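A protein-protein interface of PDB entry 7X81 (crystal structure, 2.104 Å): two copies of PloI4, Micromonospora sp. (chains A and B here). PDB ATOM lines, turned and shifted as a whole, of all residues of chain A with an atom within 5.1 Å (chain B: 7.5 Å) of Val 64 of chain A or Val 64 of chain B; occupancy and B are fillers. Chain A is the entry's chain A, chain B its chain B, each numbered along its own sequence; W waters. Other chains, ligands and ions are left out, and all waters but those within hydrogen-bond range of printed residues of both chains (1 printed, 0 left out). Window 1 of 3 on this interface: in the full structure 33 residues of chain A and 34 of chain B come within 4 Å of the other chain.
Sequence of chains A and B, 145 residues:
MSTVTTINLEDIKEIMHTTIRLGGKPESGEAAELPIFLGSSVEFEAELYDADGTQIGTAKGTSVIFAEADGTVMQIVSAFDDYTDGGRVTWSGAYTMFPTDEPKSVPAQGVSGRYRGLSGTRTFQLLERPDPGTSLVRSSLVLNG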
ATOM      1  N   GLY A  39     -23.354  27.057 -15.586  1.00  0.00           N
ATOM      2  CA  GLY A  39     -22.663  26.357 -14.509  1.00  0.00           C
ATOM      3  C   GLY A  39     -21.180  26.228 -14.791  1.00  0.00           C
ATOM      4  O   GLY A  39     -20.745  26.204 -15.953  1.00  0.00           O
ATOM      5  N   SER A  40     -20.381  26.190 -13.715  1.00  0.00           N
ATOM      6  CA  SER A  40     -18.992  25.804 -13.882  1.00  0.00           C
ATOM      7  C   SER A  40     -18.947  24.418 -14.522  1.00  0.00           C
ATOM      8  O   SER A  40     -19.752  23.539 -14.185  1.00  0.00           O
ATOM      9  CB  SER A  40     -18.260  25.783 -12.554  1.00  0.00           C
ATOM     10  OG  SER A  40     -18.263  27.051 -11.914  1.00  0.00           O
ATOM     11  N   SER A  41     -18.019  24.208 -15.446  1.00  0.00           N
ATOM     12  CA  SER A  41     -17.968  22.966 -16.204  1.00  0.00           C
ATOM     13  C   SER A  41     -16.549  22.424 -16.306  1.00  0.00           C
ATOM     14  O   SER A  41     -15.579  23.184 -16.280  1.00  0.00           O
ATOM     15  CB  SER A  41     -18.503  23.196 -17.565  1.00  0.00           C
ATOM     16  OG  SER A  41     -17.740  24.185 -18.253  1.00  0.00           O
ATOM     17  N   VAL A  42     -16.447  21.105 -16.394  1.00  0.00           N
ATOM     18  CA  VAL A  42     -15.196  20.373 -16.536  1.00  0.00           C
ATOM     19  C   VAL A  42     -15.298  19.494 -17.788  1.00  0.00           C
ATOM     20  O   VAL A  42     -16.038  18.513 -17.799  1.00  0.00           O
ATOM     21  CB  VAL A  42     -14.898  19.491 -15.316  1.00  0.00           C
ATOM     22  CG1 VAL A  42     -13.537  18.858 -15.455  1.00  0.00           C
ATOM     23  CG2 VAL A  42     -14.892  20.330 -14.007  1.00  0.00           C
ATOM     24  N   THR A  62     -18.088  15.330 -19.907  1.00  0.00           N
ATOM     25  CA  THR A  62     -18.307  16.664 -19.394  1.00  0.00           C
ATOM     26  C   THR A  62     -19.072  16.562 -18.090  1.00  0.00           C
ATOM     27  O   THR A  62     -20.006  15.755 -17.995  1.00  0.00           O
ATOM     28  CB  THR A  62     -19.112  17.474 -20.394  1.00  0.00           C
ATOM     29  OG1 THR A  62     -18.360  17.598 -21.587  1.00  0.00           O
ATOM     30  CG2 THR A  62     -19.410  18.866 -19.823  1.00  0.00           C
ATOM     31  N   SER A  63     -18.657  17.366 -17.096  1.00  0.00           N
ATOM     32  CA  SER A  63     -19.365  17.575 -15.842  1.00  0.00           C
ATOM     33  C   SER A  63     -19.722  19.058 -15.713  1.00  0.00           C
ATOM     34  O   SER A  63     -18.953  19.933 -16.137  1.00  0.00           O
ATOM     35  CB  SER A  63     -18.523  17.179 -14.616  1.00  0.00           C
ATOM     36  OG  SER A  63     -18.422  15.773 -14.483  1.00  0.00           O
ATOM     37  N   VAL A  64     -20.883  19.336 -15.102  1.00  0.00           N
ATOM     38  CA  VAL A  64     -21.337  20.715 -14.838  1.00  0.00           C
ATOM     39  C   VAL A  64     -21.900  20.770 -13.432  1.00  0.00           C
ATOM     40  O   VAL A  64     -22.565  19.836 -13.000  1.00  0.00           O
ATOM     41  CB  VAL A  64     -22.395  21.151 -15.851  1.00  0.00           C
ATOM     42  CG1 VAL A  64     -22.851  22.605 -15.603  1.00  0.00           C
ATOM     43  CG2 VAL A  64     -21.850  20.946 -17.270  1.00  0.00           C
ATOM     44  N   ILE A  65     -21.688  21.863 -12.742  1.00  0.00           N
ATOM     45  CA  ILE A  65     -22.149  22.046 -11.359  1.00  0.00           C
ATOM     46  C   ILE A  65     -23.535  22.692 -11.372  1.00  0.00           C
ATOM     47  O   ILE A  65     -23.796  23.615 -12.147  1.00  0.00           O
ATOM     48  CB  ILE A  65     -21.149  22.904 -10.532  1.00  0.00           C
ATOM     49  CG1 ILE A  65     -19.761  22.272 -10.602  1.00  0.00           C
ATOM     50  CG2 ILE A  65     -21.667  23.113  -9.117  1.00  0.00           C
ATOM     51  CD1 ILE A  65     -18.685  22.968  -9.691  1.00  0.00           C
ATOM     52  N   PHE A  66     -24.411  22.199 -10.506  1.00  0.00           N
ATOM     53  CA  PHE A  66     -25.705  22.740 -10.261  1.00  0.00           C
ATOM     54  C   PHE A  66     -26.089  22.444  -8.818  1.00  0.00           C
ATOM     55  O   PHE A  66     -25.297  21.879  -8.058  1.00  0.00           O
ATOM     56  CB  PHE A  66     -26.707  22.151 -11.260  1.00  0.00           C
ATOM     57  CG  PHE A  66     -27.108  20.732 -10.980  1.00  0.00           C
ATOM     58  CD1 PHE A  66     -26.249  19.686 -11.299  1.00  0.00           C
ATOM     59  CD2 PHE A  66     -28.347  20.434 -10.463  1.00  0.00           C
ATOM     60  CE1 PHE A  66     -26.606  18.354 -11.057  1.00  0.00           C
ATOM     61  CE2 PHE A  66     -28.749  19.124 -10.243  1.00  0.00           C
ATOM     62  CZ  PHE A  66     -27.872  18.072 -10.531  1.00  0.00           C
ATOM     63  N   MET A  74     -24.436  19.852  -6.568  1.00  0.00           N
ATOM     64  CA  MET A  74     -24.305  18.615  -7.317  1.00  0.00           C
ATOM     65  C   MET A  74     -23.426  18.842  -8.529  1.00  0.00           C
ATOM     66  O   MET A  74     -23.162  19.974  -8.919  1.00  0.00           O
ATOM     67  CB  MET A  74     -25.687  18.119  -7.786  1.00  0.00           C
ATOM     68  CG  MET A  74     -26.716  18.064  -6.689  1.00  0.00           C
ATOM     69  SD  MET A  74     -26.528  16.638  -5.583  1.00  0.00           S
ATOM     70  CE  MET A  74     -26.742  15.277  -6.684  1.00  0.00           C
ATOM     71  N   GLN A  75     -23.002  17.742  -9.152  1.00  0.00           N
ATOM     72  CA  GLN A  75     -22.459  17.781 -10.504  1.00  0.00           C
ATOM     73  C   GLN A  75     -23.221  16.770 -11.345  1.00  0.00           C
ATOM     74  O   GLN A  75     -23.661  15.743 -10.849  1.00  0.00           O
ATOM     75  CB  GLN A  75     -20.948  17.489 -10.545  1.00  0.00           C
ATOM     76  CG  GLN A  75     -20.135  18.489  -9.733  1.00  0.00           C
ATOM     77  CD  GLN A  75     -18.619  18.357  -9.902  1.00  0.00           C
ATOM     78  OE1 GLN A  75     -18.153  17.571 -10.672  1.00  0.00           O
ATOM     79  NE2 GLN A  75     -17.867  19.191  -9.203  1.00  0.00           N
ATOM     80  N   ILE A  76     -23.380  17.069 -12.622  1.00  0.00           N
ATOM     81  CA  ILE A  76     -23.987  16.146 -13.579  1.00  0.00           C
ATOM     82  C   ILE A  76     -22.922  15.814 -14.605  1.00  0.00           C
ATOM     83  O   ILE A  76     -22.183  16.700 -15.039  1.00  0.00           O
ATOM     84  CB  ILE A  76     -25.224  16.776 -14.233  1.00  0.00           C
ATOM     85  CG1 ILE A  76     -25.976  15.772 -15.095  1.00  0.00           C
ATOM     86  CG2 ILE A  76     -24.860  17.993 -15.037  1.00  0.00           C
ATOM     87  CD1 ILE A  76     -27.376  16.220 -15.434  1.00  0.00           C
ATOM     88  N   PHE B  37     -19.853  28.496 -10.080  1.00  0.00           N
ATOM     89  CA  PHE B  37     -21.224  28.947 -10.257  1.00  0.00           C
ATOM     90  C   PHE B  37     -22.125  27.722 -10.410  1.00  0.00           C
ATOM     91  O   PHE B  37     -21.729  26.718 -10.986  1.00  0.00           O
ATOM     92  CB  PHE B  37     -21.373  29.851 -11.508  1.00  0.00           C
ATOM     93  CG  PHE B  37     -21.003  31.270 -11.274  1.00  0.00           C
ATOM     94  CD1 PHE B  37     -21.950  32.169 -10.825  1.00  0.00           C
ATOM     95  CD2 PHE B  37     -19.699  31.712 -11.528  1.00  0.00           C
ATOM     96  CE1 PHE B  37     -21.624  33.500 -10.615  1.00  0.00           C
ATOM     97  CE2 PHE B  37     -19.350  33.028 -11.319  1.00  0.00           C
ATOM     98  CZ  PHE B  37     -20.300  33.934 -10.849  1.00  0.00           C
ATOM     99  N   LEU B  38     -23.332  27.806  -9.879  1.00  0.00           N
ATOM    100  CA  LEU B  38     -24.342  26.773 -10.065  1.00  0.00           C
ATOM    101  C   LEU B  38     -25.122  27.094 -11.341  1.00  0.00           C
ATOM    102  O   LEU B  38     -25.746  28.158 -11.443  1.00  0.00           O
ATOM    103  CB  LEU B  38     -25.287  26.721  -8.860  1.00  0.00           C
ATOM    104  CG  LEU B  38     -24.625  26.858  -7.490  1.00  0.00           C
ATOM    105  CD1 LEU B  38     -25.711  27.064  -6.403  1.00  0.00           C
ATOM    106  CD2 LEU B  38     -23.771  25.677  -7.133  1.00  0.00           C
ATOM    107  N   GLY B  39     -25.066  26.212 -12.315  1.00  0.00           N
ATOM    108  CA  GLY B  39     -25.801  26.452 -13.528  1.00  0.00           C
ATOM    109  C   GLY B  39     -27.291  26.295 -13.314  1.00  0.00           C
ATOM    110  O   GLY B  39     -27.767  25.618 -12.391  1.00  0.00           O
ATOM    111  N   SER B  40     -28.054  26.965 -14.169  1.00  0.00           N
ATOM    112  CA  SER B  40     -29.494  26.747 -14.202  1.00  0.00           C
ATOM    113  C   SER B  40     -29.777  25.296 -14.554  1.00  0.00           C
ATOM    114  O   SER B  40     -29.119  24.691 -15.422  1.00  0.00           O
ATOM    115  CB  SER B  40     -30.131  27.671 -15.225  1.00  0.00           C
ATOM    116  OG  SER B  40     -29.863  28.997 -14.862  1.00  0.00           O
ATOM    117  N   SER B  41     -30.774  24.741 -13.893  1.00  0.00           N
ATOM    118  CA  SER B  41     -31.107  23.336 -14.081  1.00  0.00           C
ATOM    119  C   SER B  41     -32.591  23.145 -14.344  1.00  0.00           C
ATOM    120  O   SER B  41     -33.441  23.911 -13.874  1.00  0.00           O
ATOM    121  CB  SER B  41     -30.707  22.513 -12.829  1.00  0.00           C
ATOM    122  OG  SER B  41     -31.267  23.079 -11.628  1.00  0.00           O
ATOM    123  N   VAL B  42     -32.899  22.091 -15.095  1.00  0.00           N
ATOM    124  CA  VAL B  42     -34.272  21.663 -15.313  1.00  0.00           C
ATOM    125  C   VAL B  42     -34.385  20.215 -14.876  1.00  0.00           C
ATOM    126  O   VAL B  42     -33.858  19.332 -15.553  1.00  0.00           O
ATOM    127  CB  VAL B  42     -34.698  21.794 -16.787  1.00  0.00           C
ATOM    128  CG1 VAL B  42     -36.156  21.342 -16.953  1.00  0.00           C
ATOM    129  CG2 VAL B  42     -34.498  23.220 -17.264  1.00  0.00           C
ATOM    130  N   GLU B  43     -35.073  19.954 -13.768  1.00  0.00           N
ATOM    131  CA  GLU B  43     -35.418  18.575 -13.392  1.00  0.00           C
ATOM    132  C   GLU B  43     -36.766  18.251 -14.022  1.00  0.00           C
ATOM    133  O   GLU B  43     -37.711  19.036 -13.907  1.00  0.00           O
ATOM    134  CB  GLU B  43     -35.470  18.426 -11.866  1.00  0.00           C
ATOM    135  CG  GLU B  43     -34.088  18.499 -11.188  1.00  0.00           C
ATOM    136  CD  GLU B  43     -34.107  19.266  -9.867  1.00  0.00           C
ATOM    137  OE1 GLU B  43     -35.210  19.476  -9.315  1.00  0.00           O
ATOM    138  OE2 GLU B  43     -33.023  19.659  -9.371  1.00  0.00           O
ATOM    139  N   THR B  62     -32.475  15.278 -15.689  1.00  0.00           N
ATOM    140  CA  THR B  62     -32.051  16.619 -15.338  1.00  0.00           C
ATOM    141  C   THR B  62     -31.235  17.188 -16.487  1.00  0.00           C
ATOM    142  O   THR B  62     -30.418  16.486 -17.085  1.00  0.00           O
ATOM    143  CB  THR B  62     -31.172  16.622 -14.065  1.00  0.00           C
ATOM    144  OG1 THR B  62     -31.738  15.768 -13.060  1.00  0.00           O
ATOM    145  CG2 THR B  62     -30.991  18.015 -13.574  1.00  0.00           C
ATOM    146  N   SER B  63     -31.450  18.460 -16.775  1.00  0.00           N
ATOM    147  CA  SER B  63     -30.627  19.210 -17.711  1.00  0.00           C
ATOM    148  C   SER B  63     -30.027  20.393 -16.981  1.00  0.00           C
ATOM    149  O   SER B  63     -30.673  20.982 -16.111  1.00  0.00           O
ATOM    150  CB  SER B  63     -31.431  19.742 -18.884  1.00  0.00           C
ATOM    151  OG  SER B  63     -31.686  18.683 -19.799  1.00  0.00           O
ATOM    152  N   VAL B  64     -28.805  20.762 -17.378  1.00  0.00           N
ATOM    153  CA  VAL B  64     -28.079  21.868 -16.761  1.00  0.00           C
ATOM    154  C   VAL B  64     -27.394  22.699 -17.840  1.00  0.00           C
ATOM    155  O   VAL B  64     -26.828  22.153 -18.800  1.00  0.00           O
ATOM    156  CB  VAL B  64     -27.038  21.341 -15.746  1.00  0.00           C
ATOM    157  CG1 VAL B  64     -26.289  22.491 -15.067  1.00  0.00           C
ATOM    158  CG2 VAL B  64     -27.707  20.407 -14.704  1.00  0.00           C
ATOM    159  N   ILE B  65     -27.392  24.041 -17.640  1.00  0.00           N
ATOM    160  CA  ILE B  65     -26.862  24.979 -18.629  1.00  0.00           C
ATOM    161  C   ILE B  65     -25.388  25.245 -18.373  1.00  0.00           C
ATOM    162  O   ILE B  65     -24.952  25.380 -17.223  1.00  0.00           O
ATOM    163  CB  ILE B  65     -27.666  26.288 -18.605  1.00  0.00           C
ATOM    164  CG1 ILE B  65     -29.145  26.027 -18.923  1.00  0.00           C
ATOM    165  CG2 ILE B  65     -27.120  27.257 -19.614  1.00  0.00           C
ATOM    166  CD1 ILE B  65     -30.031  27.273 -18.928  1.00  0.00           C
ATOM    167  N   PHE B  66     -24.617  25.326 -19.453  1.00  0.00           N
ATOM    168  CA  PHE B  66     -23.200  25.674 -19.370  1.00  0.00           C
ATOM    169  C   PHE B  66     -22.759  26.262 -20.708  1.00  0.00           C
ATOM    170  O   PHE B  66     -23.569  26.494 -21.617  1.00  0.00           O
ATOM    171  CB  PHE B  66     -22.349  24.457 -18.955  1.00  0.00           C
ATOM    172  CG  PHE B  66     -22.124  23.436 -20.055  1.00  0.00           C
ATOM    173  CD1 PHE B  66     -23.144  22.592 -20.456  1.00  0.00           C
ATOM    174  CD2 PHE B  66     -20.876  23.302 -20.670  1.00  0.00           C
ATOM    175  CE1 PHE B  66     -22.943  21.646 -21.456  1.00  0.00           C
ATOM    176  CE2 PHE B  66     -20.664  22.345 -21.686  1.00  0.00           C
ATOM    177  CZ  PHE B  66     -21.703  21.511 -22.067  1.00  0.00           C
ATOM    178  N   ALA B  67     -21.463  26.520 -20.832  1.00  0.00           N
ATOM    179  CA  ALA B  67     -20.960  27.080 -22.076  1.00  0.00           C
ATOM    180  C   ALA B  67     -19.611  26.464 -22.403  1.00  0.00           C
ATOM    181  O   ALA B  67     -18.812  26.147 -21.512  1.00  0.00           O
ATOM    182  CB  ALA B  67     -20.837  28.596 -22.021  1.00  0.00           C
ATOM    183  N   MET B  74     -24.772  25.813 -23.956  1.00  0.00           N
ATOM    184  CA  MET B  74     -25.181  24.452 -24.143  1.00  0.00           C
ATOM    185  C   MET B  74     -26.067  24.017 -22.985  1.00  0.00           C
ATOM    186  O   MET B  74     -26.166  24.664 -21.948  1.00  0.00           O
ATOM    187  CB  MET B  74     -23.963  23.505 -24.230  1.00  0.00           C
ATOM    188  CG  MET B  74     -22.876  23.786 -25.240  1.00  0.00           C
ATOM    189  SD  MET B  74     -23.219  23.544 -26.836  1.00  0.00           S
ATOM    190  CE  MET B  74     -23.586  21.858 -27.109  1.00  0.00           C
ATOM    191  N   GLN B  75     -26.715  22.866 -23.149  1.00  0.00           N
ATOM    192  CA  GLN B  75     -27.319  22.141 -22.042  1.00  0.00           C
ATOM    193  C   GLN B  75     -26.748  20.731 -22.039  1.00  0.00           C
ATOM    194  O   GLN B  75     -26.457  20.150 -23.096  1.00  0.00           O
ATOM    195  CB  GLN B  75     -28.852  22.126 -22.150  1.00  0.00           C
ATOM    196  CG  GLN B  75     -29.464  23.514 -22.002  1.00  0.00           C
ATOM    197  CD  GLN B  75     -30.997  23.533 -21.943  1.00  0.00           C
ATOM    198  OE1 GLN B  75     -31.648  22.514 -22.057  1.00  0.00           O
ATOM    199  NE2 GLN B  75     -31.563  24.725 -21.767  1.00  0.00           N
ATOM    200  N   ILE B  76     -26.548  20.189 -20.859  1.00  0.00           N
ATOM    201  CA  ILE B  76     -26.164  18.796 -20.727  1.00  0.00           C
ATOM    202  C   ILE B  76     -27.304  18.074 -20.039  1.00  0.00           C
ATOM    203  O   ILE B  76     -27.890  18.605 -19.100  1.00  0.00           O
ATOM    204  CB  ILE B  76     -24.848  18.630 -19.969  1.00  0.00           C
ATOM    205  CG1 ILE B  76     -24.515  17.138 -19.839  1.00  0.00           C
ATOM    206  CG2 ILE B  76     -24.926  19.296 -18.629  1.00  0.00           C
ATOM    207  CD1 ILE B  76     -23.117  16.867 -19.343  1.00  0.00           C
ATOM    208  N   VAL B  77     -27.667  16.911 -20.546  1.00  0.00           N
ATOM    209  CA  VAL B  77     -28.748  16.150 -19.941  1.00  0.00           C
ATOM    210  C   VAL B  77     -28.265  14.748 -19.565  1.00  0.00           C
ATOM    211  O   VAL B  77     -27.390  14.157 -20.209  1.00  0.00           O
ATOM    212  CB  VAL B  77     -29.981  16.079 -20.873  1.00  0.00           C
ATOM    213  CG1 VAL B  77     -29.601  15.404 -22.192  1.00  0.00           C
ATOM    214  CG2 VAL B  77     -31.113  15.328 -20.195  1.00  0.00           C
ATOM    215  N   SER B  78     -28.855  14.227 -18.489  1.00  0.00           N
ATOM    216  CA  SER B  78     -28.762  12.832 -18.102  1.00  0.00           C
ATOM    217  C   SER B  78     -30.169  12.373 -17.746  1.00  0.00           C
ATOM    218  O   SER B  78     -30.798  12.924 -16.825  1.00  0.00           O
ATOM    219  CB  SER B  78     -27.819  12.652 -16.921  1.00  0.00           C
ATOM    220  OG  SER B  78     -27.689  11.278 -16.573  1.00  0.00           O
ATOM    221  N   GLY B  93     -26.090  13.515 -22.901  1.00  0.00           N
ATOM    222  CA  GLY B  93     -25.168  14.205 -23.778  1.00  0.00           C
ATOM    223  C   GLY B  93     -25.365  15.694 -23.628  1.00  0.00           C
ATOM    224  O   GLY B  93     -26.160  16.156 -22.823  1.00  0.00           O
ATOM    225  N   ALA B  94     -24.617  16.440 -24.417  1.00  0.00           N
ATOM    226  CA  ALA B  94     -24.778  17.882 -24.454  1.00  0.00           C
ATOM    227  C   ALA B  94     -25.335  18.302 -25.809  1.00  0.00           C
ATOM    228  O   ALA B  94     -25.038  17.695 -26.834  1.00  0.00           O
ATOM    229  CB  ALA B  94     -23.453  18.590 -24.180  1.00  0.00           C
ATOM    230  N   TYR B  95     -26.154  19.350 -25.803  1.00  0.00           N
ATOM    231  CA  TYR B  95     -26.707  19.911 -27.046  1.00  0.00           C
ATOM    232  C   TYR B  95     -26.739  21.437 -26.964  1.00  0.00           C
ATOM    233  O   TYR B  95     -26.692  22.003 -25.879  1.00  0.00           O
ATOM    234  CB  TYR B  95     -28.133  19.405 -27.308  1.00  0.00           C
ATOM    235  CG  TYR B  95     -29.029  19.540 -26.102  1.00  0.00           C
ATOM    236  CD1 TYR B  95     -29.053  18.570 -25.129  1.00  0.00           C
ATOM    237  CD2 TYR B  95     -29.793  20.672 -25.914  1.00  0.00           C
ATOM    238  CE1 TYR B  95     -29.825  18.692 -24.038  1.00  0.00           C
ATOM    239  CE2 TYR B  95     -30.584  20.809 -24.820  1.00  0.00           C
ATOM    240  CZ  TYR B  95     -30.603  19.811 -23.877  1.00  0.00           C
ATOM    241  OH  TYR B  95     -31.386  19.924 -22.757  1.00  0.00           O
HETATM  242  O   HOH W   1     -19.476  26.501 -18.435  1.00  0.00           O
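The backbone carbonyl oxygen (O) of Ile 65 of chain A sits at hydrogen-bond distance from the backbone NH (N) of Gly 39 of chain B.
The side-chain hydroxyl (OG) of Ser 40 of chain A is in hydrogen-bond range of the backbone NH (N) of Phe 37 of chain B (2.8 Å).
O of Ile 65 of chain B is in hydrogen-bond range of N of Gly 39 of chain A (2.8 Å).
The backbone NH (N) of Ser 78 of chain B lies within hydrogen-bond range of the backbone carbonyl oxygen (O) of Thr 62 of chain B.
The backbone NH (N) of Met 74 of chain B is in hydrogen-bond range of the backbone carbonyl oxygen (O) of Phe 66 of chain B (2.7 Å).
N of Ile 76 of chain B lies within hydrogen-bond range of O of Val 64 of chain B (2.9 Å).
The backbone NH of Ile 76 of chain A is in hydrogen-bond range of the backbone carbonyl oxygen of Val 64 of chain A (2.9 Å).
The backbone carbonyl oxygen (O) of Ser 40 of chain B is in hydrogen-bond range of the backbone NH (N) of Ile 65 of chain B (2.9 Å).
O of Phe 66 of chain A lies within hydrogen-bond range of N of Met 74 of chain A (2.7 Å).
CB of Ser 41 of chain A touches CD2 of Phe 66 of chain B, at 3.9 Å.
Ser 41 of chain A touches Ala 67 of chain B.
Val 64 of chain A touches Val 64 of chain B (CG1 to CG1, 3.5 Å).
Val 64 of chain A touches Ile 65 of chain B (CG1 to O, 3.8 Å).
CG2 of Ile 76 of chain B touches CG2 of Val 64 of chain A, 3.7 Å away.
Phe 37 of chain B touches Ile 65 of chain A.
O of Gly 39 of chain B touches CB of Phe 66 of chain A (3.8 Å).
Val 64 of chain B touches Phe 66 of chain A.
CD1 of Ile 76 of chain A touches O of Thr 62 of chain B, at 3.5 Å.
Ile 76 of chain A touches Ile 76 of chain B (CG2 to CG2, 3.8 Å).
Of chain B, only Val 64 (3.5 Å), Ile 65 (3.8 Å), Phe 66 (3.7 Å) and Ile 76 (3.7 Å) come within 4 Å of Val 64 of chain A.
Printed residues of chain A within 4 Å of Val 64 of chain B: Val 64 (3.5 Å), Phe 66 (3.8 Å) and Ile 76 (3.7 Å).
Of the printed residues of chain B, Ser 40 of chain A touches Phe 37.
Printed residues of chain B within 4 Å of Phe 66 of chain A: Gly 39 (3.8 Å), Ser 41 (3.9 Å) and Val 64 (3.8 Å).
Printed residues of chain B within 4 Å of Thr 62 of chain A: Ile 76.
Ser 63 of chain A touches none of the printed residues of chain B.
Ser 40 of chain B touches none of the printed residues of chain A.
The nearest residue of chain B that does not touch Val 64 of chain A is Gly 39 of chain B (5.3 Å).
The nearest printed residue of chain A that does not touch Val 64 of chain B is Ile 65 of chain A (4.001 Å).
The nearest printed residue of chain B that does not touch Thr 62 of chain A is Phe 66 of chain B (4.1 Å).
Of the 12 printed residues of chain A, 8 touch a printed residue of chain B.
Hydrophobic or aromatic side chains of chain A that line the printed part of chain B: Val 64, Ile 65, Phe 66 and Ile 76.
Along chain A the printed residues that touch a printed residue of chain B span positions 39 to 76.
Of the 21 printed residues of chain B, 11 touch a printed residue of chain A.
Hydrophobic or aromatic side chains of chain B that line the printed part of chain A: Leu 38, Val 64, Phe 66 and Ile 76.
Along chain B the printed residues that touch a printed residue of chain A span positions 37 to 78.
Gly 39 of chain A touches Phe 66 of chain B, and with the chains exchanged Phe 66 of chain A touches Gly 39 of chain B.
Ser 41 of chain A touches Phe 66 of chain B, and with the chains exchanged Phe 66 of chain A touches Ser 41 of chain B.
Thr 62 of chain A touches Ile 76 of chain B, and with the chains exchanged Ile 76 of chain A touches Thr 62 of chain B.
Ile 76 of chain A touches its own counterpart, Ile 76 of chain B.
Water W1 lies within hydrogen-bond range of the backbone carbonyl oxygen (O) of Gly 39 of chain A, the side-chain hydroxyl (OG) of Ser 41 of chain A and the backbone NH (N) of Ala 67 of chain B.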
